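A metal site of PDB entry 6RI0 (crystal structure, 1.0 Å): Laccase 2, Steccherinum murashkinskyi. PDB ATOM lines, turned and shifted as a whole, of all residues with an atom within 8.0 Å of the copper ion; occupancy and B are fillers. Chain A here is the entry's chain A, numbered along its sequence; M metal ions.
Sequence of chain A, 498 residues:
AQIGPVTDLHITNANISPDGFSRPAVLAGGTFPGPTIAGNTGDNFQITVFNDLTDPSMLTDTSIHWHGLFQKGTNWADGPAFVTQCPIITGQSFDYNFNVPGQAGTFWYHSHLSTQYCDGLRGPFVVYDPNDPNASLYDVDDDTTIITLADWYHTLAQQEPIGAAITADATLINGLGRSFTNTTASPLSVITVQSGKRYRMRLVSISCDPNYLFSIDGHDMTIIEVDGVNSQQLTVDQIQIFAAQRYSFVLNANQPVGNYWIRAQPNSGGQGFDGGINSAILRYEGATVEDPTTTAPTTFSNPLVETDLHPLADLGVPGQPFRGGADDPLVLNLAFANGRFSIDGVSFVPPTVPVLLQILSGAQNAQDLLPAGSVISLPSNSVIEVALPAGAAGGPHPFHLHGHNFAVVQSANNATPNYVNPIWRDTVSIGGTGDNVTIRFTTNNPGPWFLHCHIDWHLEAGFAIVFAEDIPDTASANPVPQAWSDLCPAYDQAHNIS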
ATOM      1  N   CYS A 208     -20.374  23.419  -1.599  1.00  0.00           N
ATOM      2  CA  CYS A 208     -20.862  22.404  -0.642  1.00  0.00           C
ATOM      3  C   CYS A 208     -22.230  21.884  -0.987  1.00  0.00           C
ATOM      4  O   CYS A 208     -22.665  20.875  -0.389  1.00  0.00           O
ATOM      5  CB  CYS A 208     -20.886  22.912   0.763  1.00  0.00           C
ATOM      6  SG  CYS A 208     -19.345  22.498   1.659  1.00  0.00           S
ATOM      7  N   ASP A 209     -22.978  22.559  -1.883  1.00  0.00           N
ATOM      8  CA  ASP A 209     -24.377  22.139  -2.116  1.00  0.00           C
ATOM      9  C   ASP A 209     -24.890  22.615  -3.461  1.00  0.00           C
ATOM     10  O   ASP A 209     -25.104  21.794  -4.337  1.00  0.00           O
ATOM     11  CB  ASP A 209     -25.241  22.514  -0.931  1.00  0.00           C
ATOM     12  CG  ASP A 209     -26.698  22.252  -1.084  1.00  0.00           C
ATOM     13  OD1 ASP A 209     -27.191  21.946  -2.138  1.00  0.00           O
ATOM     14  OD2 ASP A 209     -27.406  22.563  -0.091  1.00  0.00           O
ATOM     15  N   PHE A 341     -29.589   9.581   4.588  1.00  0.00           N
ATOM     16  CA  PHE A 341     -29.451   8.934   3.312  1.00  0.00           C
ATOM     17  C   PHE A 341     -28.976   7.523   3.515  1.00  0.00           C
ATOM     18  O   PHE A 341     -28.286   7.192   4.467  1.00  0.00           O
ATOM     19  CB  PHE A 341     -28.463   9.693   2.436  1.00  0.00           C
ATOM     20  CG  PHE A 341     -28.991  11.012   1.937  1.00  0.00           C
ATOM     21  CD1 PHE A 341     -28.761  12.180   2.615  1.00  0.00           C
ATOM     22  CD2 PHE A 341     -29.732  11.075   0.777  1.00  0.00           C
ATOM     23  CE1 PHE A 341     -29.241  13.384   2.151  1.00  0.00           C
ATOM     24  CE2 PHE A 341     -30.239  12.272   0.322  1.00  0.00           C
ATOM     25  CZ  PHE A 341     -30.000  13.435   1.014  1.00  0.00           C
ATOM     26  N   ALA A 392     -34.275  10.103  -4.585  1.00  0.00           N
ATOM     27  CA  ALA A 392     -34.024  10.518  -3.175  1.00  0.00           C
ATOM     28  C   ALA A 392     -34.175  12.012  -3.062  1.00  0.00           C
ATOM     29  O   ALA A 392     -33.642  12.765  -3.901  1.00  0.00           O
ATOM     30  CB  ALA A 392     -32.641  10.075  -2.736  1.00  0.00           C
ATOM     31  N   ALA A 393     -34.790  12.467  -1.958  1.00  0.00           N
ATOM     32  CA  ALA A 393     -34.965  13.881  -1.675  1.00  0.00           C
ATOM     33  C   ALA A 393     -33.638  14.611  -1.698  1.00  0.00           C
ATOM     34  O   ALA A 393     -32.559  14.065  -1.471  1.00  0.00           O
ATOM     35  CB  ALA A 393     -35.608  14.015  -0.301  1.00  0.00           C
ATOM     36  N   GLY A 394     -33.750  15.909  -1.968  1.00  0.00           N
ATOM     37  CA  GLY A 394     -32.611  16.805  -1.951  1.00  0.00           C
ATOM     38  C   GLY A 394     -31.833  16.863  -3.239  1.00  0.00           C
ATOM     39  O   GLY A 394     -30.749  17.423  -3.254  1.00  0.00           O
ATOM     40  N   GLY A 395     -32.398  16.300  -4.294  1.00  0.00           N
ATOM     41  CA  GLY A 395     -31.667  16.271  -5.594  1.00  0.00           C
ATOM     42  C   GLY A 395     -31.712  17.623  -6.288  1.00  0.00           C
ATOM     43  O   GLY A 395     -32.369  18.570  -5.843  1.00  0.00           O
ATOM     44  N   PRO A 396     -30.986  17.745  -7.421  1.00  0.00           N
ATOM     45  CA  PRO A 396     -30.275  16.656  -8.086  1.00  0.00           C
ATOM     46  C   PRO A 396     -28.911  16.444  -7.419  1.00  0.00           C
ATOM     47  O   PRO A 396     -28.161  17.364  -7.115  1.00  0.00           O
ATOM     48  CB  PRO A 396     -30.115  17.181  -9.498  1.00  0.00           C
ATOM     49  CG  PRO A 396     -30.140  18.679  -9.352  1.00  0.00           C
ATOM     50  CD  PRO A 396     -31.083  18.960  -8.227  1.00  0.00           C
ATOM     51  N   HIS A 397     -28.603  15.160  -7.200  1.00  0.00           N
ATOM     52  CA  HIS A 397     -27.418  14.771  -6.431  1.00  0.00           C
ATOM     53  C   HIS A 397     -26.226  14.585  -7.360  1.00  0.00           C
ATOM     54  O   HIS A 397     -26.277  13.742  -8.264  1.00  0.00           O
ATOM     55  CB  HIS A 397     -27.656  13.452  -5.672  1.00  0.00           C
ATOM     56  CG  HIS A 397     -28.807  13.517  -4.741  1.00  0.00           C
ATOM     57  ND1 HIS A 397     -28.701  14.157  -3.499  1.00  0.00           N
ATOM     58  CD2 HIS A 397     -30.063  13.024  -4.846  1.00  0.00           C
ATOM     59  CE1 HIS A 397     -29.891  14.052  -2.939  1.00  0.00           C
ATOM     60  NE2 HIS A 397     -30.707  13.374  -3.693  1.00  0.00           N
ATOM     61  N   PRO A 398     -25.102  15.312  -7.105  1.00  0.00           N
ATOM     62  CA  PRO A 398     -23.882  15.112  -7.895  1.00  0.00           C
ATOM     63  C   PRO A 398     -22.996  14.053  -7.304  1.00  0.00           C
ATOM     64  O   PRO A 398     -22.253  14.278  -6.342  1.00  0.00           O
ATOM     65  CB  PRO A 398     -23.241  16.493  -7.875  1.00  0.00           C
ATOM     66  CG  PRO A 398     -23.634  17.030  -6.518  1.00  0.00           C
ATOM     67  CD  PRO A 398     -24.993  16.488  -6.239  1.00  0.00           C
ATOM     68  N   PHE A 399     -23.062  12.840  -7.847  1.00  0.00           N
ATOM     69  CA  PHE A 399     -22.264  11.734  -7.349  1.00  0.00           C
ATOM     70  C   PHE A 399     -20.853  11.771  -7.893  1.00  0.00           C
ATOM     71  O   PHE A 399     -20.603  12.032  -9.070  1.00  0.00           O
ATOM     72  CB  PHE A 399     -22.937  10.366  -7.664  1.00  0.00           C
ATOM     73  CG  PHE A 399     -23.810   9.910  -6.534  1.00  0.00           C
ATOM     74  CD1 PHE A 399     -24.996  10.530  -6.247  1.00  0.00           C
ATOM     75  CD2 PHE A 399     -23.394   8.867  -5.700  1.00  0.00           C
ATOM     76  CE1 PHE A 399     -25.738  10.165  -5.119  1.00  0.00           C
ATOM     77  CE2 PHE A 399     -24.113   8.504  -4.602  1.00  0.00           C
ATOM     78  CZ  PHE A 399     -25.303   9.135  -4.307  1.00  0.00           C
ATOM     79  N   ILE A 430     -27.099  12.956 -10.986  1.00  0.00           N
ATOM     80  CA  ILE A 430     -27.961  11.806 -11.245  1.00  0.00           C
ATOM     81  C   ILE A 430     -29.365  12.188 -11.620  1.00  0.00           C
ATOM     82  O   ILE A 430     -30.200  11.322 -11.916  1.00  0.00           O
ATOM     83  CB  ILE A 430     -27.903  10.759 -10.133  1.00  0.00           C
ATOM     84  CG1 ILE A 430     -28.596  11.219  -8.867  1.00  0.00           C
ATOM     85  CG2 ILE A 430     -26.457  10.313  -9.876  1.00  0.00           C
ATOM     86  CD1 ILE A 430     -28.744  10.127  -7.833  1.00  0.00           C
ATOM     87  N   HIS A 452     -19.794   8.937  -3.394  1.00  0.00           N
ATOM     88  CA  HIS A 452     -20.747   9.648  -2.562  1.00  0.00           C
ATOM     89  C   HIS A 452     -21.329  10.810  -3.303  1.00  0.00           C
ATOM     90  O   HIS A 452     -20.776  11.319  -4.256  1.00  0.00           O
ATOM     91  CB  HIS A 452     -20.101  10.115  -1.247  1.00  0.00           C
ATOM     92  CG  HIS A 452     -18.968  11.085  -1.433  1.00  0.00           C
ATOM     93  ND1 HIS A 452     -19.112  12.435  -1.522  1.00  0.00           N
ATOM     94  CD2 HIS A 452     -17.644  10.863  -1.487  1.00  0.00           C
ATOM     95  CE1 HIS A 452     -17.914  12.984  -1.646  1.00  0.00           C
ATOM     96  NE2 HIS A 452     -16.979  12.064  -1.623  1.00  0.00           N
ATOM     97  N   CYS A 453     -22.480  11.286  -2.802  1.00  0.00           N
ATOM     98  CA  CYS A 453     -22.998  12.591  -3.225  1.00  0.00           C
ATOM     99  C   CYS A 453     -22.051  13.676  -2.748  1.00  0.00           C
ATOM    100  O   CYS A 453     -21.638  13.640  -1.575  1.00  0.00           O
ATOM    101  CB  CYS A 453     -24.398  12.819  -2.633  1.00  0.00           C
ATOM    102  SG  CYS A 453     -25.030  14.414  -3.223  1.00  0.00           S
ATOM    103  N   HIS A 454     -21.709  14.620  -3.624  1.00  0.00           N
ATOM    104  CA  HIS A 454     -20.795  15.689  -3.258  1.00  0.00           C
ATOM    105  C   HIS A 454     -21.470  16.896  -2.656  1.00  0.00           C
ATOM    106  O   HIS A 454     -20.806  17.882  -2.336  1.00  0.00           O
ATOM    107  CB  HIS A 454     -19.894  16.066  -4.441  1.00  0.00           C
ATOM    108  CG  HIS A 454     -18.491  16.446  -4.032  1.00  0.00           C
ATOM    109  ND1 HIS A 454     -18.205  17.521  -3.254  1.00  0.00           N
ATOM    110  CD2 HIS A 454     -17.293  15.885  -4.333  1.00  0.00           C
ATOM    111  CE1 HIS A 454     -16.876  17.564  -3.067  1.00  0.00           C
ATOM    112  NE2 HIS A 454     -16.284  16.603  -3.721  1.00  0.00           N
ATOM    113  N   ILE A 455     -22.789  16.842  -2.418  1.00  0.00           N
ATOM    114  CA  ILE A 455     -23.426  17.829  -1.540  1.00  0.00           C
ATOM    115  C   ILE A 455     -22.967  17.424  -0.118  1.00  0.00           C
ATOM    116  O   ILE A 455     -23.309  16.334   0.371  1.00  0.00           O
ATOM    117  CB  ILE A 455     -24.942  17.825  -1.697  1.00  0.00           C
ATOM    118  CG1 ILE A 455     -25.309  18.331  -3.103  1.00  0.00           C
ATOM    119  CG2 ILE A 455     -25.579  18.691  -0.617  1.00  0.00           C
ATOM    120  CD1 ILE A 455     -26.761  18.117  -3.532  1.00  0.00           C
ATOM    121  N   ASP A 456     -22.153  18.268   0.484  1.00  0.00           N
ATOM    122  CA  ASP A 456     -21.440  17.827   1.672  1.00  0.00           C
ATOM    123  C   ASP A 456     -22.385  17.536   2.811  1.00  0.00           C
ATOM    124  O   ASP A 456     -22.122  16.661   3.648  1.00  0.00           O
ATOM    125  CB  ASP A 456     -20.394  18.894   2.056  1.00  0.00           C
ATOM    126  CG  ASP A 456     -19.111  18.311   2.663  1.00  0.00           C
ATOM    127  OD1 ASP A 456     -18.743  17.191   2.258  1.00  0.00           O
ATOM    128  OD2 ASP A 456     -18.507  18.986   3.484  1.00  0.00           O
ATOM    129  N   TRP A 457     -23.523  18.245   2.863  1.00  0.00           N
ATOM    130  CA  TRP A 457     -24.532  17.984   3.873  1.00  0.00           C
ATOM    131  C   TRP A 457     -25.142  16.579   3.723  1.00  0.00           C
ATOM    132  O   TRP A 457     -25.541  15.953   4.704  1.00  0.00           O
ATOM    133  CB  TRP A 457     -25.647  19.072   3.826  1.00  0.00           C
ATOM    134  CG  TRP A 457     -25.093  20.465   3.717  1.00  0.00           C
ATOM    135  CD1 TRP A 457     -25.206  21.311   2.648  1.00  0.00           C
ATOM    136  CD2 TRP A 457     -24.347  21.169   4.698  1.00  0.00           C
ATOM    137  NE1 TRP A 457     -24.570  22.483   2.904  1.00  0.00           N
ATOM    138  CE2 TRP A 457     -24.012  22.439   4.150  1.00  0.00           C
ATOM    139  CE3 TRP A 457     -23.923  20.877   5.991  1.00  0.00           C
ATOM    140  CZ2 TRP A 457     -23.289  23.371   4.839  1.00  0.00           C
ATOM    141  CZ3 TRP A 457     -23.235  21.796   6.640  1.00  0.00           C
ATOM    142  CH2 TRP A 457     -22.883  23.038   6.090  1.00  0.00           C
ATOM    143  N   HIS A 458     -25.190  16.080   2.501  1.00  0.00           N
ATOM    144  CA  HIS A 458     -25.739  14.750   2.220  1.00  0.00           C
ATOM    145  C   HIS A 458     -24.709  13.657   2.543  1.00  0.00           C
ATOM    146  O   HIS A 458     -25.086  12.617   3.072  1.00  0.00           O
ATOM    147  CB  HIS A 458     -26.197  14.665   0.771  1.00  0.00           C
ATOM    148  CG  HIS A 458     -27.275  15.619   0.405  1.00  0.00           C
ATOM    149  ND1 HIS A 458     -27.748  15.690  -0.889  1.00  0.00           N
ATOM    150  CD2 HIS A 458     -27.967  16.479   1.191  1.00  0.00           C
ATOM    151  CE1 HIS A 458     -28.715  16.608  -0.860  1.00  0.00           C
ATOM    152  NE2 HIS A 458     -28.879  17.094   0.364  1.00  0.00           N
ATOM    153  N   LEU A 459     -23.441  13.903   2.208  1.00  0.00           N
ATOM    154  CA  LEU A 459     -22.379  13.010   2.619  1.00  0.00           C
ATOM    155  C   LEU A 459     -22.415  12.863   4.129  1.00  0.00           C
ATOM    156  O   LEU A 459     -22.366  11.722   4.671  1.00  0.00           O
ATOM    157  CB  LEU A 459     -21.061  13.516   2.165  1.00  0.00           C
ATOM    158  CG  LEU A 459     -19.804  12.812   2.700  1.00  0.00           C
ATOM    159  CD1 LEU A 459     -19.813  11.340   2.394  1.00  0.00           C
ATOM    160  CD2 LEU A 459     -18.530  13.479   2.183  1.00  0.00           C
ATOM    161  N   PHE A 463     -24.802   9.627   2.683  1.00  0.00           N
ATOM    162  CA  PHE A 463     -25.034   9.260   1.266  1.00  0.00           C
ATOM    163  C   PHE A 463     -23.724   8.835   0.577  1.00  0.00           C
ATOM    164  O   PHE A 463     -23.186   9.543  -0.271  1.00  0.00           O
ATOM    165  CB  PHE A 463     -25.717  10.412   0.541  1.00  0.00           C
ATOM    166  CG  PHE A 463     -26.667  10.039  -0.571  1.00  0.00           C
ATOM    167  CD1 PHE A 463     -27.159   8.750  -0.778  1.00  0.00           C
ATOM    168  CD2 PHE A 463     -27.155  11.044  -1.387  1.00  0.00           C
ATOM    169  CE1 PHE A 463     -28.112   8.493  -1.723  1.00  0.00           C
ATOM    170  CE2 PHE A 463     -28.123  10.788  -2.367  1.00  0.00           C
ATOM    171  CZ  PHE A 463     -28.615   9.526  -2.508  1.00  0.00           C
HETATM  172 CU    CU M   1     -27.054  14.731  -2.494  1.00  0.00          CU
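The backbone carbonyl oxygen of His 458 is in hydrogen-bond range of the backbone NH of Phe 463 (3.0 Å). The backbone carbonyl oxygen of Ala 393 lies within hydrogen-bond range of a ring nitrogen (NE2) of His 397. A ring nitrogen (NE2) of His 397 sits at hydrogen-bond distance from the backbone NH (N) of Gly 395, 3.4 Å away. NE2 of His 397 lies within hydrogen-bond range of O of Ala 392 (3.0 Å). The backbone carbonyl oxygen (O) of His 397 is in hydrogen-bond range of the backbone NH (N) of Ile 430 (3.0 Å). The side-chain sulfur of Cys 453 sits close to the backbone NH of Ile 455 (3.4 Å). The backbone NH (N) of Cys 453 is in hydrogen-bond range of the backbone carbonyl oxygen (O) of Phe 463, at 3.2 Å.
The copper ion is bound by a ring nitrogen (ND1) of His 458 (2.0 Å), a ring nitrogen (ND1) of His 397 (2.0 Å) and the side-chain sulfur of Cys 453 (2.2 Å).
Residues that only touch the copper ion: Ile 455 (3.6 Å) and Phe 463 (3.9 Å). Five residues have an atom within 4 Å of the copper ion: His 397, Cys 453, Ile 455, His 458 and Phe 463. The nearest printed residue that does not touch the copper ion is Pro 398 (4.6 Å).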
